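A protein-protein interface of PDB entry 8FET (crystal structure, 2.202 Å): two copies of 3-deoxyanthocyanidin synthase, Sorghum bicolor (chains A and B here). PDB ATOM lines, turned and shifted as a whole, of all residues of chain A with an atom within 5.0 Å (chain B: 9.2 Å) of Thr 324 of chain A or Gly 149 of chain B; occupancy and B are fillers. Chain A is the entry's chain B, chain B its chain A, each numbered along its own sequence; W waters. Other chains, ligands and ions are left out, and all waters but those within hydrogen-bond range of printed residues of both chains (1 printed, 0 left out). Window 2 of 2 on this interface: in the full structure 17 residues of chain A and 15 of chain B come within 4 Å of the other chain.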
ATOM      1  N   TYR A 273      -8.657  22.959 -33.904  1.00  0.00           N
ATOM      2  CA  TYR A 273      -8.000  22.315 -32.764  1.00  0.00           C
ATOM      3  C   TYR A 273      -6.583  22.858 -32.597  1.00  0.00           C
ATOM      4  O   TYR A 273      -5.822  22.913 -33.568  1.00  0.00           O
ATOM      5  CB  TYR A 273      -7.976  20.775 -32.905  1.00  0.00           C
ATOM      6  CG  TYR A 273      -7.797  20.118 -31.557  1.00  0.00           C
ATOM      7  CD1 TYR A 273      -6.534  19.966 -31.007  1.00  0.00           C
ATOM      8  CD2 TYR A 273      -8.891  19.714 -30.803  1.00  0.00           C
ATOM      9  CE1 TYR A 273      -6.360  19.406 -29.758  1.00  0.00           C
ATOM     10  CE2 TYR A 273      -8.727  19.148 -29.546  1.00  0.00           C
ATOM     11  CZ  TYR A 273      -7.456  18.997 -29.034  1.00  0.00           C
ATOM     12  OH  TYR A 273      -7.278  18.437 -27.791  1.00  0.00           O
ATOM     13  N   HIS A 322     -15.042  18.092 -37.916  1.00  0.00           N
ATOM     14  CA  HIS A 322     -13.886  17.437 -37.298  1.00  0.00           C
ATOM     15  C   HIS A 322     -13.453  18.264 -36.091  1.00  0.00           C
ATOM     16  O   HIS A 322     -12.740  19.262 -36.233  1.00  0.00           O
ATOM     17  CB  HIS A 322     -12.773  17.275 -38.324  1.00  0.00           C
ATOM     18  CG  HIS A 322     -13.231  16.606 -39.577  1.00  0.00           C
ATOM     19  ND1 HIS A 322     -12.980  15.277 -39.846  1.00  0.00           N
ATOM     20  CD2 HIS A 322     -13.960  17.071 -40.619  1.00  0.00           C
ATOM     21  CE1 HIS A 322     -13.515  14.961 -41.013  1.00  0.00           C
ATOM     22  NE2 HIS A 322     -14.118  16.030 -41.499  1.00  0.00           N
ATOM     23  N   ASN A 323     -13.879  17.842 -34.897  1.00  0.00           N
ATOM     24  CA  ASN A 323     -13.777  18.689 -33.720  1.00  0.00           C
ATOM     25  C   ASN A 323     -12.819  18.192 -32.649  1.00  0.00           C
ATOM     26  O   ASN A 323     -12.434  18.981 -31.784  1.00  0.00           O
ATOM     27  CB  ASN A 323     -15.167  18.889 -33.109  1.00  0.00           C
ATOM     28  CG  ASN A 323     -16.118  19.540 -34.092  1.00  0.00           C
ATOM     29  OD1 ASN A 323     -15.943  20.703 -34.450  1.00  0.00           O
ATOM     30  ND2 ASN A 323     -17.106  18.786 -34.563  1.00  0.00           N
ATOM     31  N   THR A 324     -12.423  16.930 -32.682  1.00  0.00           N
ATOM     32  CA  THR A 324     -11.416  16.404 -31.774  1.00  0.00           C
ATOM     33  C   THR A 324     -10.113  16.247 -32.542  1.00  0.00           C
ATOM     34  O   THR A 324     -10.093  16.239 -33.774  1.00  0.00           O
ATOM     35  CB  THR A 324     -11.831  15.048 -31.180  1.00  0.00           C
ATOM     36  OG1 THR A 324     -11.967  14.085 -32.234  1.00  0.00           O
ATOM     37  CG2 THR A 324     -13.155  15.155 -30.419  1.00  0.00           C
ATOM     38  N   LEU A 325      -9.011  16.140 -31.797  1.00  0.00           N
ATOM     39  CA  LEU A 325      -7.731  15.943 -32.460  1.00  0.00           C
ATOM     40  C   LEU A 325      -7.786  14.710 -33.345  1.00  0.00           C
ATOM     41  O   LEU A 325      -7.249  14.703 -34.461  1.00  0.00           O
ATOM     42  CB  LEU A 325      -6.612  15.825 -31.425  1.00  0.00           C
ATOM     43  CG  LEU A 325      -5.172  15.852 -31.953  1.00  0.00           C
ATOM     44  CD1 LEU A 325      -4.950  16.904 -33.043  1.00  0.00           C
ATOM     45  CD2 LEU A 325      -4.207  16.085 -30.805  1.00  0.00           C
ATOM     46  N   GLU A 326      -8.472  13.670 -32.873  1.00  0.00           N
ATOM     47  CA  GLU A 326      -8.520  12.415 -33.607  1.00  0.00           C
ATOM     48  C   GLU A 326      -9.339  12.537 -34.884  1.00  0.00           C
ATOM     49  O   GLU A 326      -8.960  11.984 -35.922  1.00  0.00           O
ATOM     50  CB  GLU A 326      -9.081  11.315 -32.719  1.00  0.00           C
ATOM     51  CG  GLU A 326      -8.737   9.949 -33.231  1.00  0.00           C
ATOM     52  CD  GLU A 326      -9.212   8.886 -32.299  1.00  0.00           C
ATOM     53  OE1 GLU A 326      -9.681   9.263 -31.204  1.00  0.00           O
ATOM     54  OE2 GLU A 326      -9.112   7.694 -32.657  1.00  0.00           O
ATOM     55  N   GLU A 327     -10.474  13.238 -34.835  1.00  0.00           N
ATOM     56  CA  GLU A 327     -11.233  13.453 -36.066  1.00  0.00           C
ATOM     57  C   GLU A 327     -10.451  14.310 -37.051  1.00  0.00           C
ATOM     58  O   GLU A 327     -10.571  14.122 -38.267  1.00  0.00           O
ATOM     59  CB  GLU A 327     -12.588  14.091 -35.752  1.00  0.00           C
ATOM     60  CG  GLU A 327     -13.515  13.181 -34.927  1.00  0.00           C
ATOM     61  CD  GLU A 327     -14.700  13.927 -34.316  1.00  0.00           C
ATOM     62  OE1 GLU A 327     -14.717  15.172 -34.375  1.00  0.00           O
ATOM     63  OE2 GLU A 327     -15.613  13.270 -33.767  1.00  0.00           O
ATOM     64  N   ILE A 328      -9.640  15.251 -36.557  1.00  0.00           N
ATOM     65  CA  ILE A 328      -8.839  16.046 -37.481  1.00  0.00           C
ATOM     66  C   ILE A 328      -7.798  15.174 -38.168  1.00  0.00           C
ATOM     67  O   ILE A 328      -7.479  15.387 -39.345  1.00  0.00           O
ATOM     68  CB  ILE A 328      -8.215  17.244 -36.746  1.00  0.00           C
ATOM     69  CG1 ILE A 328      -9.203  18.414 -36.742  1.00  0.00           C
ATOM     70  CG2 ILE A 328      -6.930  17.648 -37.414  1.00  0.00           C
ATOM     71  CD1 ILE A 328      -9.060  19.277 -35.529  1.00  0.00           C
ATOM     72  N   LEU B 143     -18.275   7.352 -22.011  1.00  0.00           N
ATOM     73  CA  LEU B 143     -17.229   8.035 -22.763  1.00  0.00           C
ATOM     74  C   LEU B 143     -15.930   8.158 -21.985  1.00  0.00           C
ATOM     75  O   LEU B 143     -14.861   7.882 -22.533  1.00  0.00           O
ATOM     76  CB  LEU B 143     -17.712   9.433 -23.184  1.00  0.00           C
ATOM     77  CG  LEU B 143     -19.011   9.541 -24.000  1.00  0.00           C
ATOM     78  CD1 LEU B 143     -19.377  10.999 -24.228  1.00  0.00           C
ATOM     79  CD2 LEU B 143     -18.918   8.829 -25.337  1.00  0.00           C
ATOM     80  N   LEU B 144     -15.986   8.545 -20.711  1.00  0.00           N
ATOM     81  CA  LEU B 144     -14.785   8.572 -19.880  1.00  0.00           C
ATOM     82  C   LEU B 144     -14.197   7.165 -19.763  1.00  0.00           C
ATOM     83  O   LEU B 144     -14.929   6.186 -19.611  1.00  0.00           O
ATOM     84  CB  LEU B 144     -15.121   9.137 -18.501  1.00  0.00           C
ATOM     85  CG  LEU B 144     -15.841  10.491 -18.525  1.00  0.00           C
ATOM     86  CD1 LEU B 144     -16.253  10.949 -17.131  1.00  0.00           C
ATOM     87  CD2 LEU B 144     -14.959  11.546 -19.188  1.00  0.00           C
ATOM     88  N   GLY B 145     -12.863   7.058 -19.842  1.00  0.00           N
ATOM     89  CA  GLY B 145     -12.209   5.762 -19.941  1.00  0.00           C
ATOM     90  C   GLY B 145     -12.046   5.242 -21.352  1.00  0.00           C
ATOM     91  O   GLY B 145     -11.275   4.303 -21.567  1.00  0.00           O
ATOM     92  N   ASP B 146     -12.748   5.845 -22.315  1.00  0.00           N
ATOM     93  CA  ASP B 146     -12.638   5.542 -23.741  1.00  0.00           C
ATOM     94  C   ASP B 146     -11.212   5.527 -24.272  1.00  0.00           C
ATOM     95  O   ASP B 146     -10.939   4.880 -25.292  1.00  0.00           O
ATOM     96  CB  ASP B 146     -13.412   6.606 -24.533  1.00  0.00           C
ATOM     97  CG  ASP B 146     -14.347   6.018 -25.524  1.00  0.00           C
ATOM     98  OD1 ASP B 146     -14.649   4.810 -25.392  1.00  0.00           O
ATOM     99  OD2 ASP B 146     -14.782   6.755 -26.433  1.00  0.00           O
ATOM    100  N   GLY B 147     -10.318   6.305 -23.669  1.00  0.00           N
ATOM    101  CA  GLY B 147      -9.054   6.649 -24.297  1.00  0.00           C
ATOM    102  C   GLY B 147      -9.136   7.712 -25.384  1.00  0.00           C
ATOM    103  O   GLY B 147      -8.095   8.119 -25.911  1.00  0.00           O
ATOM    104  N   HIS B 148     -10.327   8.172 -25.749  1.00  0.00           N
ATOM    105  CA  HIS B 148     -10.473   9.170 -26.795  1.00  0.00           C
ATOM    106  C   HIS B 148     -10.814  10.526 -26.194  1.00  0.00           C
ATOM    107  O   HIS B 148     -11.306  10.629 -25.063  1.00  0.00           O
ATOM    108  CB  HIS B 148     -11.565   8.775 -27.791  1.00  0.00           C
ATOM    109  CG  HIS B 148     -11.315   7.473 -28.482  1.00  0.00           C
ATOM    110  ND1 HIS B 148     -10.173   7.221 -29.209  1.00  0.00           N
ATOM    111  CD2 HIS B 148     -12.055   6.342 -28.536  1.00  0.00           C
ATOM    112  CE1 HIS B 148     -10.228   5.995 -29.698  1.00  0.00           C
ATOM    113  NE2 HIS B 148     -11.359   5.440 -29.301  1.00  0.00           N
ATOM    114  N   GLY B 149     -10.543  11.577 -26.972  1.00  0.00           N
ATOM    115  CA  GLY B 149     -11.017  12.888 -26.604  1.00  0.00           C
ATOM    116  C   GLY B 149     -12.465  13.079 -27.008  1.00  0.00           C
ATOM    117  O   GLY B 149     -12.988  12.374 -27.865  1.00  0.00           O
ATOM    118  N   HIS B 150     -13.130  14.040 -26.369  1.00  0.00           N
ATOM    119  CA  HIS B 150     -14.547  14.249 -26.617  1.00  0.00           C
ATOM    120  C   HIS B 150     -14.877  15.718 -26.411  1.00  0.00           C
ATOM    121  O   HIS B 150     -14.333  16.356 -25.509  1.00  0.00           O
ATOM    122  CB  HIS B 150     -15.414  13.385 -25.685  1.00  0.00           C
ATOM    123  CG  HIS B 150     -15.256  11.910 -25.894  1.00  0.00           C
ATOM    124  ND1 HIS B 150     -15.853  11.237 -26.939  1.00  0.00           N
ATOM    125  CD2 HIS B 150     -14.576  10.975 -25.184  1.00  0.00           C
ATOM    126  CE1 HIS B 150     -15.543   9.955 -26.869  1.00  0.00           C
ATOM    127  NE2 HIS B 150     -14.772   9.769 -25.812  1.00  0.00           N
ATOM    128  N   VAL B 151     -15.759  16.249 -27.255  1.00  0.00           N
ATOM    129  CA  VAL B 151     -16.342  17.568 -27.050  1.00  0.00           C
ATOM    130  C   VAL B 151     -17.777  17.341 -26.596  1.00  0.00           C
ATOM    131  O   VAL B 151     -18.629  16.935 -27.396  1.00  0.00           O
ATOM    132  CB  VAL B 151     -16.284  18.432 -28.320  1.00  0.00           C
ATOM    133  CG1 VAL B 151     -16.750  19.852 -28.014  1.00  0.00           C
ATOM    134  CG2 VAL B 151     -14.875  18.459 -28.878  1.00  0.00           C
ATOM    135  N   LEU B 152     -18.058  17.580 -25.320  1.00  0.00           N
ATOM    136  CA  LEU B 152     -19.413  17.410 -24.818  1.00  0.00           C
ATOM    137  C   LEU B 152     -20.224  18.691 -25.022  1.00  0.00           C
ATOM    138  O   LEU B 152     -19.709  19.801 -24.854  1.00  0.00           O
ATOM    139  CB  LEU B 152     -19.389  17.034 -23.338  1.00  0.00           C
ATOM    140  CG  LEU B 152     -18.519  15.829 -22.961  1.00  0.00           C
ATOM    141  CD1 LEU B 152     -18.703  15.455 -21.494  1.00  0.00           C
ATOM    142  CD2 LEU B 152     -18.838  14.643 -23.849  1.00  0.00           C
ATOM    143  N   THR B 239      -9.618  13.492 -14.762  1.00  0.00           N
ATOM    144  CA  THR B 239     -10.818  13.023 -15.452  1.00  0.00           C
ATOM    145  C   THR B 239     -10.951  13.584 -16.865  1.00  0.00           C
ATOM    146  O   THR B 239     -11.324  12.853 -17.790  1.00  0.00           O
ATOM    147  CB  THR B 239     -12.057  13.401 -14.648  1.00  0.00           C
ATOM    148  OG1 THR B 239     -12.028  12.719 -13.397  1.00  0.00           O
ATOM    149  CG2 THR B 239     -13.304  13.011 -15.403  1.00  0.00           C
ATOM    150  N   SER B 240     -10.689  14.881 -17.057  1.00  0.00           N
ATOM    151  CA  SER B 240     -10.965  15.532 -18.332  1.00  0.00           C
ATOM    152  C   SER B 240      -9.727  16.022 -19.077  1.00  0.00           C
ATOM    153  O   SER B 240      -9.862  16.490 -20.215  1.00  0.00           O
ATOM    154  CB  SER B 240     -11.944  16.693 -18.115  1.00  0.00           C
ATOM    155  OG  SER B 240     -13.098  16.216 -17.435  1.00  0.00           O
ATOM    156  N   GLY B 241      -8.535  15.917 -18.489  1.00  0.00           N
ATOM    157  CA  GLY B 241      -7.314  16.337 -19.154  1.00  0.00           C
ATOM    158  C   GLY B 241      -7.056  17.831 -19.131  1.00  0.00           C
ATOM    159  O   GLY B 241      -6.118  18.293 -19.797  1.00  0.00           O
ATOM    160  N   GLU B 242      -7.843  18.585 -18.368  1.00  0.00           N
ATOM    161  CA  GLU B 242      -7.881  20.046 -18.334  1.00  0.00           C
ATOM    162  C   GLU B 242      -8.880  20.424 -17.243  1.00  0.00           C
ATOM    163  O   GLU B 242      -9.636  19.578 -16.756  1.00  0.00           O
ATOM    164  CB  GLU B 242      -8.298  20.636 -19.691  1.00  0.00           C
ATOM    165  CG  GLU B 242      -9.819  20.554 -19.924  1.00  0.00           C
ATOM    166  CD  GLU B 242     -10.257  20.797 -21.364  1.00  0.00           C
ATOM    167  OE1 GLU B 242      -9.413  20.726 -22.284  1.00  0.00           O
ATOM    168  OE2 GLU B 242     -11.463  21.082 -21.578  1.00  0.00           O
ATOM    169  N   ARG B 303      -3.370  13.962 -21.226  1.00  0.00           N
ATOM    170  CA  ARG B 303      -4.533  13.087 -21.303  1.00  0.00           C
ATOM    171  C   ARG B 303      -5.416  13.478 -22.475  1.00  0.00           C
ATOM    172  O   ARG B 303      -5.410  14.635 -22.907  1.00  0.00           O
ATOM    173  CB  ARG B 303      -5.352  13.159 -20.020  1.00  0.00           C
ATOM    174  CG  ARG B 303      -4.522  12.996 -18.789  1.00  0.00           C
ATOM    175  CD  ARG B 303      -5.354  13.125 -17.550  1.00  0.00           C
ATOM    176  NE  ARG B 303      -4.546  12.821 -16.378  1.00  0.00           N
ATOM    177  CZ  ARG B 303      -4.049  11.625 -16.096  1.00  0.00           C
ATOM    178  NH1 ARG B 303      -4.287  10.575 -16.871  1.00  0.00           N
ATOM    179  NH2 ARG B 303      -3.308  11.474 -14.999  1.00  0.00           N
ATOM    180  N   PRO B 304      -6.187  12.540 -23.018  1.00  0.00           N
ATOM    181  CA  PRO B 304      -7.216  12.938 -23.979  1.00  0.00           C
ATOM    182  C   PRO B 304      -8.139  13.948 -23.314  1.00  0.00           C
ATOM    183  O   PRO B 304      -8.409  13.875 -22.114  1.00  0.00           O
ATOM    184  CB  PRO B 304      -7.919  11.618 -24.322  1.00  0.00           C
ATOM    185  CG  PRO B 304      -6.877  10.554 -24.003  1.00  0.00           C
ATOM    186  CD  PRO B 304      -6.186  11.085 -22.779  1.00  0.00           C
ATOM    187  N   ARG B 305      -8.556  14.945 -24.084  1.00  0.00           N
ATOM    188  CA  ARG B 305      -9.313  16.055 -23.531  1.00  0.00           C
ATOM    189  C   ARG B 305     -10.795  15.750 -23.668  1.00  0.00           C
ATOM    190  O   ARG B 305     -11.288  15.503 -24.772  1.00  0.00           O
ATOM    191  CB  ARG B 305      -8.964  17.372 -24.229  1.00  0.00           C
ATOM    192  CG  ARG B 305      -7.472  17.725 -24.211  1.00  0.00           C
ATOM    193  CD  ARG B 305      -7.086  18.584 -23.007  1.00  0.00           C
ATOM    194  NE  ARG B 305      -5.803  19.265 -23.179  1.00  0.00           N
ATOM    195  CZ  ARG B 305      -5.635  20.580 -23.087  1.00  0.00           C
ATOM    196  NH1 ARG B 305      -6.655  21.395 -22.856  1.00  0.00           N
ATOM    197  NH2 ARG B 305      -4.415  21.093 -23.237  1.00  0.00           N
ATOM    198  N   VAL B 306     -11.497  15.753 -22.546  1.00  0.00           N
ATOM    199  CA  VAL B 306     -12.952  15.713 -22.536  1.00  0.00           C
ATOM    200  C   VAL B 306     -13.398  17.123 -22.169  1.00  0.00           C
ATOM    201  O   VAL B 306     -13.414  17.495 -20.995  1.00  0.00           O
ATOM    202  CB  VAL B 306     -13.484  14.656 -21.564  1.00  0.00           C
ATOM    203  CG1 VAL B 306     -15.005  14.689 -21.534  1.00  0.00           C
ATOM    204  CG2 VAL B 306     -12.976  13.287 -21.991  1.00  0.00           C
ATOM    205  N   THR B 307     -13.739  17.916 -23.177  1.00  0.00           N
ATOM    206  CA  THR B 307     -13.912  19.349 -23.014  1.00  0.00           C
ATOM    207  C   THR B 307     -15.366  19.744 -23.274  1.00  0.00           C
ATOM    208  O   THR B 307     -16.200  18.932 -23.689  1.00  0.00           O
ATOM    209  CB  THR B 307     -12.941  20.110 -23.933  1.00  0.00           C
ATOM    210  OG1 THR B 307     -12.883  21.478 -23.528  1.00  0.00           O
ATOM    211  CG2 THR B 307     -13.368  20.024 -25.406  1.00  0.00           C
HETATM  212  O   HOH W   1     -12.353  11.603 -31.084  1.00  0.00           O
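A ring nitrogen (ND1) of His 148 of chain B sits at hydrogen-bond distance from the side-chain carboxylate (OE1) of Glu 326 of chain A (2.9 Å).
NH1 of Arg 305 of chain B lies within salt-bridge range of OE1 of Glu 242 of chain B (2.9 Å).
The backbone NH (N) of Glu 327 of chain A sits at hydrogen-bond distance from the side-chain hydroxyl (OG1) of Thr 324 of chain A (3.1 Å).
The backbone NH (N) of His 150 of chain B sits at hydrogen-bond distance from the backbone carbonyl oxygen (O) of Arg 305 of chain B.
N of Asn 323 of chain A sits at hydrogen-bond distance from OE1 of Glu 327 of chain A (2.8 Å).
Among the printed residues, pairs that only touch across the chains: Tyr 273 of chain A with Arg 305 of chain B (3.7 Å), Asn 323 of chain A with Val 151 of chain B (3.8 Å) and Thr 324 of chain A with Gly 149 of chain B (3.8 Å).
Of the printed residues of chain B, Tyr 273 of chain A touches Arg 305 (3.7 Å).
His 322 of chain A touches none of the printed residues of chain B.
Of chain B, only Gly 149 (3.8 Å) comes within 4 Å of Thr 324 of chain A.
Of the printed residues of chain B, Glu 326 of chain A touches His 148 (2.9 Å).
No residue of chain B comes within 4 Å of Glu 327 of chain A.
Of the printed residues of chain A, His 148 of chain B touches Glu 326.
Of the printed residues of chain A, Gly 149 of chain B touches Thr 324.
Of the printed residues of chain A, Val 151 of chain B touches Asn 323 (3.8 Å).
The nearest printed residue of chain B that does not touch Asn 323 of chain A is Thr 307 of chain B (6.5 Å).
Printed residues of chain B that touch a printed residue of chain A: His 148, Gly 149, Val 151 and Arg 305.
Of the 8 printed residues of chain A, 4 touch a printed residue of chain B.
Among the printed residues, 4 pairs touch across the chains.
No position is printed for both chains.
Water W1 lies within hydrogen-bond range of the side-chain hydroxyl (OG1) of Thr 324 of chain A and the backbone carbonyl oxygen (O) of Gly 149 of chain B.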
